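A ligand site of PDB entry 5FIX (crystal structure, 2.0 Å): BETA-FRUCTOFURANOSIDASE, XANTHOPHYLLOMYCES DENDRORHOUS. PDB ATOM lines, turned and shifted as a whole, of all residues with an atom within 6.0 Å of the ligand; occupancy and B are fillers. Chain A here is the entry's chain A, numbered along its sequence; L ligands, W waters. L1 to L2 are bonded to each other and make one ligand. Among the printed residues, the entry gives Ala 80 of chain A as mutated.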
ATOM      1  N   ASN A  79       8.517 -14.126 -20.344  1.00  0.00           N
ATOM      2  CA  ASN A  79       7.872 -13.266 -21.317  1.00  0.00           C
ATOM      3  C   ASN A  79       6.599 -12.620 -20.731  1.00  0.00           C
ATOM      4  O   ASN A  79       6.719 -11.901 -19.730  1.00  0.00           O
ATOM      5  CB  ASN A  79       7.747 -13.919 -22.743  1.00  0.00           C
ATOM      6  CG  ASN A  79       6.994 -15.246 -22.794  1.00  0.00           C
ATOM      7  OD1 ASN A  79       7.428 -16.255 -22.241  1.00  0.00           O
ATOM      8  ND2 ASN A  79       5.876 -15.258 -23.515  1.00  0.00           N
ATOM      9  N   ALA A  80       5.429 -12.846 -21.319  1.00  0.00           N
ATOM     10  CA  ALA A  80       4.210 -12.085 -21.040  1.00  0.00           C
ATOM     11  C   ALA A  80       3.794 -12.077 -19.565  1.00  0.00           C
ATOM     12  O   ALA A  80       3.801 -13.114 -18.917  1.00  0.00           O
ATOM     13  CB  ALA A  80       3.067 -12.654 -21.860  1.00  0.00           C
ATOM     14  N   GLN A  97       4.792 -15.527 -17.782  1.00  0.00           N
ATOM     15  CA  GLN A  97       5.257 -16.667 -18.534  1.00  0.00           C
ATOM     16  C   GLN A  97       6.758 -16.894 -18.174  1.00  0.00           C
ATOM     17  O   GLN A  97       7.550 -15.955 -18.283  1.00  0.00           O
ATOM     18  CB  GLN A  97       5.104 -16.402 -20.030  1.00  0.00           C
ATOM     19  CG  GLN A  97       3.656 -16.319 -20.473  1.00  0.00           C
ATOM     20  CD  GLN A  97       3.024 -17.678 -20.623  1.00  0.00           C
ATOM     21  OE1 GLN A  97       3.130 -18.294 -21.692  1.00  0.00           O
ATOM     22  NE2 GLN A  97       2.327 -18.142 -19.580  1.00  0.00           N
ATOM     23  N   TRP A 105      12.341 -19.886 -24.569  1.00  0.00           N
ATOM     24  CA  TRP A 105      10.985 -20.286 -24.194  1.00  0.00           C
ATOM     25  C   TRP A 105      10.799 -21.813 -24.179  1.00  0.00           C
ATOM     26  O   TRP A 105      11.412 -22.529 -24.966  1.00  0.00           O
ATOM     27  CB  TRP A 105      10.026 -19.627 -25.194  1.00  0.00           C
ATOM     28  CG  TRP A 105       8.542 -19.822 -25.040  1.00  0.00           C
ATOM     29  CD1 TRP A 105       7.663 -18.964 -24.458  1.00  0.00           C
ATOM     30  CD2 TRP A 105       7.767 -20.896 -25.575  1.00  0.00           C
ATOM     31  NE1 TRP A 105       6.386 -19.457 -24.551  1.00  0.00           N
ATOM     32  CE2 TRP A 105       6.422 -20.637 -25.257  1.00  0.00           C
ATOM     33  CE3 TRP A 105       8.083 -22.058 -26.306  1.00  0.00           C
ATOM     34  CZ2 TRP A 105       5.383 -21.489 -25.622  1.00  0.00           C
ATOM     35  CZ3 TRP A 105       7.053 -22.901 -26.681  1.00  0.00           C
ATOM     36  CH2 TRP A 105       5.718 -22.621 -26.344  1.00  0.00           C
ATOM     37  N   ILE A 108       6.147 -23.746 -20.758  1.00  0.00           N
ATOM     38  CA  ILE A 108       5.904 -22.403 -20.259  1.00  0.00           C
ATOM     39  C   ILE A 108       4.928 -22.487 -19.074  1.00  0.00           C
ATOM     40  O   ILE A 108       3.948 -23.230 -19.125  1.00  0.00           O
ATOM     41  CB  ILE A 108       5.534 -21.413 -21.381  1.00  0.00           C
ATOM     42  CG1 ILE A 108       5.907 -19.968 -20.993  1.00  0.00           C
ATOM     43  CG2 ILE A 108       4.062 -21.518 -21.783  1.00  0.00           C
ATOM     44  CD1 ILE A 108       7.410 -19.690 -20.911  1.00  0.00           C
ATOM     45  N   VAL A 144       1.413 -23.836 -20.241  1.00  0.00           N
ATOM     46  CA  VAL A 144       0.445 -22.997 -19.588  1.00  0.00           C
ATOM     47  C   VAL A 144       0.669 -21.575 -20.099  1.00  0.00           C
ATOM     48  O   VAL A 144       1.534 -20.841 -19.595  1.00  0.00           O
ATOM     49  CB  VAL A 144       0.593 -23.068 -18.043  1.00  0.00           C
ATOM     50  CG1 VAL A 144      -0.319 -22.065 -17.349  1.00  0.00           C
ATOM     51  CG2 VAL A 144       0.288 -24.474 -17.573  1.00  0.00           C
ATOM     52  N   PHE A 145      -0.102 -21.202 -21.114  1.00  0.00           N
ATOM     53  CA  PHE A 145       0.014 -19.914 -21.796  1.00  0.00           C
ATOM     54  C   PHE A 145      -0.719 -18.838 -20.968  1.00  0.00           C
ATOM     55  O   PHE A 145      -1.100 -19.077 -19.820  1.00  0.00           O
ATOM     56  CB  PHE A 145      -0.568 -20.009 -23.228  1.00  0.00           C
ATOM     57  CG  PHE A 145       0.341 -20.669 -24.242  1.00  0.00           C
ATOM     58  CD1 PHE A 145       1.272 -21.635 -23.906  1.00  0.00           C
ATOM     59  CD2 PHE A 145       0.178 -20.346 -25.590  1.00  0.00           C
ATOM     60  CE1 PHE A 145       2.051 -22.256 -24.870  1.00  0.00           C
ATOM     61  CE2 PHE A 145       0.956 -20.959 -26.575  1.00  0.00           C
ATOM     62  CZ  PHE A 145       1.897 -21.913 -26.210  1.00  0.00           C
ATOM     63  N   ASP A 146      -0.829 -17.629 -21.524  1.00  0.00           N
ATOM     64  CA  ASP A 146      -1.435 -16.468 -20.851  1.00  0.00           C
ATOM     65  C   ASP A 146      -2.853 -16.762 -20.352  1.00  0.00           C
ATOM     66  O   ASP A 146      -3.586 -17.567 -20.933  1.00  0.00           O
ATOM     67  CB  ASP A 146      -1.459 -15.311 -21.856  1.00  0.00           C
ATOM     68  CG  ASP A 146      -1.791 -13.954 -21.236  1.00  0.00           C
ATOM     69  OD1 ASP A 146      -1.715 -13.745 -20.007  1.00  0.00           O
ATOM     70  OD2 ASP A 146      -2.136 -13.047 -22.054  1.00  0.00           O
ATOM     71  N   THR A 163      -4.874 -20.242 -21.336  1.00  0.00           N
ATOM     72  CA  THR A 163      -4.741 -21.103 -22.501  1.00  0.00           C
ATOM     73  C   THR A 163      -3.902 -22.333 -22.171  1.00  0.00           C
ATOM     74  O   THR A 163      -2.711 -22.231 -21.856  1.00  0.00           O
ATOM     75  CB  THR A 163      -4.185 -20.361 -23.709  1.00  0.00           C
ATOM     76  OG1 THR A 163      -5.079 -19.305 -24.079  1.00  0.00           O
ATOM     77  CG2 THR A 163      -3.989 -21.310 -24.870  1.00  0.00           C
ATOM     78  N   LEU A 170       1.495 -25.244 -33.796  1.00  0.00           N
ATOM     79  CA  LEU A 170       0.930 -24.129 -33.071  1.00  0.00           C
ATOM     80  C   LEU A 170       1.629 -22.864 -33.577  1.00  0.00           C
ATOM     81  O   LEU A 170       2.857 -22.731 -33.445  1.00  0.00           O
ATOM     82  CB  LEU A 170       1.151 -24.321 -31.560  1.00  0.00           C
ATOM     83  CG  LEU A 170       0.326 -23.440 -30.580  1.00  0.00           C
ATOM     84  CD1 LEU A 170       0.436 -23.980 -29.159  1.00  0.00           C
ATOM     85  CD2 LEU A 170       0.753 -21.977 -30.623  1.00  0.00           C
ATOM     86  N   GLY A 171       0.857 -21.968 -34.180  1.00  0.00           N
ATOM     87  CA  GLY A 171       1.386 -20.695 -34.635  1.00  0.00           C
ATOM     88  C   GLY A 171       0.598 -20.118 -35.772  1.00  0.00           C
ATOM     89  O   GLY A 171      -0.010 -20.850 -36.558  1.00  0.00           O
ATOM     90  N   ALA A 172       0.639 -18.790 -35.875  1.00  0.00           N
ATOM     91  CA  ALA A 172      -0.113 -18.055 -36.870  1.00  0.00           C
ATOM     92  C   ALA A 172       0.321 -18.351 -38.310  1.00  0.00           C
ATOM     93  O   ALA A 172      -0.492 -18.235 -39.231  1.00  0.00           O
ATOM     94  CB  ALA A 172      -0.003 -16.563 -36.582  1.00  0.00           C
ATOM     95  N   ARG A 220      -6.138 -18.062 -28.265  1.00  0.00           N
ATOM     96  CA  ARG A 220      -5.496 -17.982 -26.963  1.00  0.00           C
ATOM     97  C   ARG A 220      -5.637 -16.645 -26.254  1.00  0.00           C
ATOM     98  O   ARG A 220      -6.191 -15.690 -26.812  1.00  0.00           O
ATOM     99  CB  ARG A 220      -3.998 -18.317 -27.117  1.00  0.00           C
ATOM    100  CG  ARG A 220      -3.193 -17.412 -28.035  1.00  0.00           C
ATOM    101  CD  ARG A 220      -1.692 -17.692 -27.903  1.00  0.00           C
ATOM    102  NE  ARG A 220      -0.920 -17.087 -28.984  1.00  0.00           N
ATOM    103  CZ  ARG A 220      -0.850 -17.564 -30.231  1.00  0.00           C
ATOM    104  NH1 ARG A 220      -1.471 -18.693 -30.574  1.00  0.00           N
ATOM    105  NH2 ARG A 220      -0.167 -16.913 -31.154  1.00  0.00           N
ATOM    106  N   ASP A 221      -5.125 -16.623 -25.027  1.00  0.00           N
ATOM    107  CA  ASP A 221      -4.991 -15.432 -24.202  1.00  0.00           C
ATOM    108  C   ASP A 221      -6.352 -14.906 -23.759  1.00  0.00           C
ATOM    109  O   ASP A 221      -6.688 -13.738 -24.020  1.00  0.00           O
ATOM    110  CB  ASP A 221      -4.159 -14.344 -24.900  1.00  0.00           C
ATOM    111  CG  ASP A 221      -2.788 -14.851 -25.375  1.00  0.00           C
ATOM    112  OD1 ASP A 221      -2.343 -15.913 -24.880  1.00  0.00           O
ATOM    113  OD2 ASP A 221      -2.206 -14.190 -26.248  1.00  0.00           O
ATOM    114  N   PHE A 302      -4.054 -11.672 -33.651  1.00  0.00           N
ATOM    115  CA  PHE A 302      -3.993 -10.930 -32.380  1.00  0.00           C
ATOM    116  C   PHE A 302      -3.495 -11.827 -31.274  1.00  0.00           C
ATOM    117  O   PHE A 302      -3.691 -13.035 -31.286  1.00  0.00           O
ATOM    118  CB  PHE A 302      -5.364 -10.394 -31.927  1.00  0.00           C
ATOM    119  CG  PHE A 302      -5.925  -9.264 -32.765  1.00  0.00           C
ATOM    120  CD1 PHE A 302      -5.108  -8.333 -33.404  1.00  0.00           C
ATOM    121  CD2 PHE A 302      -7.301  -9.108 -32.852  1.00  0.00           C
ATOM    122  CE1 PHE A 302      -5.675  -7.299 -34.157  1.00  0.00           C
ATOM    123  CE2 PHE A 302      -7.869  -8.073 -33.595  1.00  0.00           C
ATOM    124  CZ  PHE A 302      -7.051  -7.163 -34.233  1.00  0.00           C
ATOM    125  N   GLU A 303      -2.873 -11.193 -30.282  1.00  0.00           N
ATOM    126  CA  GLU A 303      -2.442 -11.846 -29.068  1.00  0.00           C
ATOM    127  C   GLU A 303      -2.647 -10.916 -27.886  1.00  0.00           C
ATOM    128  O   GLU A 303      -2.683  -9.694 -28.052  1.00  0.00           O
ATOM    129  CB  GLU A 303      -0.951 -12.218 -29.151  1.00  0.00           C
ATOM    130  CG  GLU A 303      -0.587 -13.122 -30.316  1.00  0.00           C
ATOM    131  CD  GLU A 303       0.893 -13.451 -30.331  1.00  0.00           C
ATOM    132  OE1 GLU A 303       1.726 -12.527 -30.369  1.00  0.00           O
ATOM    133  OE2 GLU A 303       1.227 -14.644 -30.349  1.00  0.00           O
ATOM    134  N   THR A 304      -2.757 -11.516 -26.710  1.00  0.00           N
ATOM    135  CA  THR A 304      -2.874 -10.838 -25.414  1.00  0.00           C
ATOM    136  C   THR A 304      -3.838  -9.654 -25.431  1.00  0.00           C
ATOM    137  O   THR A 304      -3.571  -8.641 -24.817  1.00  0.00           O
ATOM    138  CB  THR A 304      -1.499 -10.404 -24.819  1.00  0.00           C
ATOM    139  OG1 THR A 304      -0.990  -9.234 -25.498  1.00  0.00           O
ATOM    140  CG2 THR A 304      -0.478 -11.521 -24.896  1.00  0.00           C
ATOM    141  N   GLU A 334       0.753  -9.813 -34.826  1.00  0.00           N
ATOM    142  CA  GLU A 334       1.869 -10.570 -35.355  1.00  0.00           C
ATOM    143  C   GLU A 334       1.951 -10.461 -36.884  1.00  0.00           C
ATOM    144  O   GLU A 334       0.922 -10.428 -37.558  1.00  0.00           O
ATOM    145  CB  GLU A 334       1.695 -12.064 -35.081  1.00  0.00           C
ATOM    146  CG  GLU A 334       1.320 -12.458 -33.664  1.00  0.00           C
ATOM    147  CD  GLU A 334       1.724 -13.895 -33.409  1.00  0.00           C
ATOM    148  OE1 GLU A 334       2.924 -14.104 -33.097  1.00  0.00           O
ATOM    149  OE2 GLU A 334       0.858 -14.780 -33.553  1.00  0.00           O
ATOM    150  N   HIS A 343       6.188  -7.889 -34.057  1.00  0.00           N
ATOM    151  CA  HIS A 343       5.171  -7.652 -33.020  1.00  0.00           C
ATOM    152  C   HIS A 343       4.881  -6.173 -32.758  1.00  0.00           C
ATOM    153  O   HIS A 343       5.793  -5.407 -32.437  1.00  0.00           O
ATOM    154  CB  HIS A 343       5.652  -8.267 -31.708  1.00  0.00           C
ATOM    155  CG  HIS A 343       5.345  -9.722 -31.575  1.00  0.00           C
ATOM    156  ND1 HIS A 343       6.098 -10.568 -30.784  1.00  0.00           N
ATOM    157  CD2 HIS A 343       4.382 -10.501 -32.125  1.00  0.00           C
ATOM    158  CE1 HIS A 343       5.602 -11.788 -30.843  1.00  0.00           C
ATOM    159  NE2 HIS A 343       4.553 -11.773 -31.646  1.00  0.00           N
ATOM    160  N   TYR A 376       6.015  -5.831 -25.635  1.00  0.00           N
ATOM    161  CA  TYR A 376       4.880  -6.565 -26.176  1.00  0.00           C
ATOM    162  C   TYR A 376       4.110  -7.206 -25.023  1.00  0.00           C
ATOM    163  O   TYR A 376       4.581  -7.211 -23.895  1.00  0.00           O
ATOM    164  CB  TYR A 376       5.372  -7.654 -27.122  1.00  0.00           C
ATOM    165  CG  TYR A 376       4.319  -8.265 -28.021  1.00  0.00           C
ATOM    166  CD1 TYR A 376       3.628  -7.504 -28.948  1.00  0.00           C
ATOM    167  CD2 TYR A 376       4.029  -9.633 -27.963  1.00  0.00           C
ATOM    168  CE1 TYR A 376       2.685  -8.059 -29.791  1.00  0.00           C
ATOM    169  CE2 TYR A 376       3.076 -10.207 -28.795  1.00  0.00           C
ATOM    170  CZ  TYR A 376       2.414  -9.426 -29.724  1.00  0.00           C
ATOM    171  OH  TYR A 376       1.481  -9.960 -30.568  1.00  0.00           O
ATOM    172  N   ALA A 377       2.931  -7.728 -25.334  1.00  0.00           N
ATOM    173  CA  ALA A 377       2.154  -8.562 -24.410  1.00  0.00           C
ATOM    174  C   ALA A 377       1.723  -7.758 -23.219  1.00  0.00           C
ATOM    175  O   ALA A 377       1.857  -8.193 -22.085  1.00  0.00           O
ATOM    176  CB  ALA A 377       2.944  -9.809 -23.998  1.00  0.00           C
ATOM    177  N   TRP A 393       5.901  -6.633 -21.364  1.00  0.00           N
ATOM    178  CA  TRP A 393       7.163  -7.366 -21.324  1.00  0.00           C
ATOM    179  C   TRP A 393       8.155  -6.696 -22.251  1.00  0.00           C
ATOM    180  O   TRP A 393       7.826  -6.438 -23.404  1.00  0.00           O
ATOM    181  CB  TRP A 393       6.900  -8.810 -21.754  1.00  0.00           C
ATOM    182  CG  TRP A 393       8.067  -9.599 -22.331  1.00  0.00           C
ATOM    183  CD1 TRP A 393       9.234  -9.942 -21.712  1.00  0.00           C
ATOM    184  CD2 TRP A 393       8.112 -10.219 -23.620  1.00  0.00           C
ATOM    185  NE1 TRP A 393      10.017 -10.695 -22.539  1.00  0.00           N
ATOM    186  CE2 TRP A 393       9.351 -10.889 -23.714  1.00  0.00           C
ATOM    187  CE3 TRP A 393       7.231 -10.253 -24.702  1.00  0.00           C
ATOM    188  CZ2 TRP A 393       9.720 -11.602 -24.860  1.00  0.00           C
ATOM    189  CZ3 TRP A 393       7.600 -10.956 -25.839  1.00  0.00           C
ATOM    190  CH2 TRP A 393       8.839 -11.615 -25.913  1.00  0.00           C
HETATM  191  C1  LIG L   1       4.053 -16.090 -28.060  1.00  0.00           C
HETATM  192  C2  LIG L   1       4.345 -15.640 -29.510  1.00  0.00           C
HETATM  193  C3  LIG L   1       3.609 -16.498 -30.518  1.00  0.00           C
HETATM  194  C4  LIG L   1       3.893 -17.960 -30.290  1.00  0.00           C
HETATM  195  C5  LIG L   1       3.528 -18.333 -28.864  1.00  0.00           C
HETATM  196  C6  LIG L   1       3.883 -19.779 -28.558  1.00  0.00           C
HETATM  197  O1  LIG L   1       3.984 -14.269 -29.712  1.00  0.00           O
HETATM  198  O2  LIG L   1       3.995 -16.107 -31.835  1.00  0.00           O
HETATM  199  O3  LIG L   1       3.126 -18.734 -31.212  1.00  0.00           O
HETATM  200  O4  LIG L   1       4.224 -17.501 -27.934  1.00  0.00           O
HETATM  201  O5  LIG L   1       5.288 -20.001 -28.788  1.00  0.00           O
HETATM  202  C1  LG2 L   2       2.682 -13.479 -26.669  1.00  0.00           C
HETATM  203  C2  LG2 L   2       2.457 -14.988 -26.474  1.00  0.00           C
HETATM  204  C3  LG2 L   2       1.007 -15.196 -26.020  1.00  0.00           C
HETATM  205  C4  LG2 L   2       1.082 -16.572 -25.394  1.00  0.00           C
HETATM  206  C5  LG2 L   2       2.448 -16.515 -24.708  1.00  0.00           C
HETATM  207  C6  LG2 L   2       3.187 -17.855 -24.691  1.00  0.00           C
HETATM  208  O1  LG2 L   2       3.948 -13.194 -27.257  1.00  0.00           O
HETATM  209  O2  LG2 L   2       2.707 -15.767 -27.666  1.00  0.00           O
HETATM  210  O3  LG2 L   2       0.051 -15.051 -27.081  1.00  0.00           O
HETATM  211  O4  LG2 L   2       0.039 -16.842 -24.449  1.00  0.00           O
HETATM  212  O5  LG2 L   2       3.193 -15.497 -25.371  1.00  0.00           O
HETATM  213  O6  LG2 L   2       4.334 -17.774 -23.824  1.00  0.00           O
HETATM  214  O   HOH W   1       4.309 -20.892 -32.096  1.00  0.00           O
HETATM  215  O   HOH W   2       1.711 -17.319 -33.541  1.00  0.00           O
HETATM  216  O   HOH W   3       7.426 -18.175 -27.865  1.00  0.00           O
HETATM  217  O   HOH W   4       5.911 -22.293 -30.000  1.00  0.00           O
HETATM  218  O   HOH W   5       5.223 -12.883 -24.991  1.00  0.00           O
HETATM  219  O   HOH W   6       6.075 -17.265 -33.221  1.00  0.00           O
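The side-chain amide oxygen of Gln 97 lies within hydrogen-bond range of an oxygen (O6) of LG2 L2 (2.5 Å). The indole nitrogen of Trp 105 sits at hydrogen-bond distance from an oxygen (O6) of LG2 L2. The side-chain carboxylate of Glu 334 sits at hydrogen-bond distance from an oxygen (O2) of LIG L1 (2.6 Å). An oxygen (O1) of LIG L1 lies within hydrogen-bond range of the side-chain carboxylate (OE2) of Glu 303, 2.9 Å away. An oxygen (O3) of LG2 L2 is in hydrogen-bond range of the guanidinium group of Arg 220, at 3.0 Å. O6 of LG2 L2 lies within hydrogen-bond range of ND2 of Asn 79, 3.0 Å away. O4 of LG2 L2 lies within hydrogen-bond range of N of Asp 146. NE2 of His 343 lies close to O1 of LIG L1, 3.2 Å away. O3 of LG2 L2 sits at hydrogen-bond distance from OD2 of Asp 221 (2.6 Å).
Water W1 bridges O3 of LIG L1 (2.6 Å) and O of Leu 170 (2.7 Å). Water W5 lies within hydrogen-bond range of an oxygen (O1) of LG2 L2 (2.6 Å) and the side-chain amide nitrogen of Asn 79 (2.9 Å). Water W2 lies within hydrogen-bond range of the side-chain carboxylate of Glu 334 (2.7 Å), the backbone NH of Ala 172 (3.0 Å), the guanidinium group of Arg 220 (3.1 Å) and an oxygen (O3) of LIG L1 (3.1 Å).
The side-chain carboxylate of Glu 334 is in hydrogen-bond range of a ring nitrogen (NE2) of His 343, 3.2 Å away. N of Thr 304 sits at hydrogen-bond distance from OD2 of Asp 221, 2.8 Å away. N of Thr 163 sits at hydrogen-bond distance from O of Asp 146 (3.0 Å). N of Gln 97 lies within hydrogen-bond range of O of Ala 80 (2.8 Å). NH2 of Arg 220 lies within salt-bridge range of OE2 of Glu 334, at 3.4 Å. N of Asp 221 sits at hydrogen-bond distance from OG1 of Thr 163 (2.8 Å). OE2 of Glu 303 lies within salt-bridge range of NH2 of Arg 220. The side-chain carboxylate (OE1) of Glu 303 sits at hydrogen-bond distance from a ring nitrogen (NE2) of His 343.
Ile 108 touches the ligand. CB of Phe 145 touches O4 of LG2 L2 (3.4 Å). CE2 of Tyr 376 touches O1 of LG2 L2 (3.5 Å). Hydrophobic or aromatic side chains that line the ligand: Trp 105, Ile 108, Phe 145, His 343 and Tyr 376. The nearest printed residue that does not touch the ligand is Leu 170 (4.1 Å).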
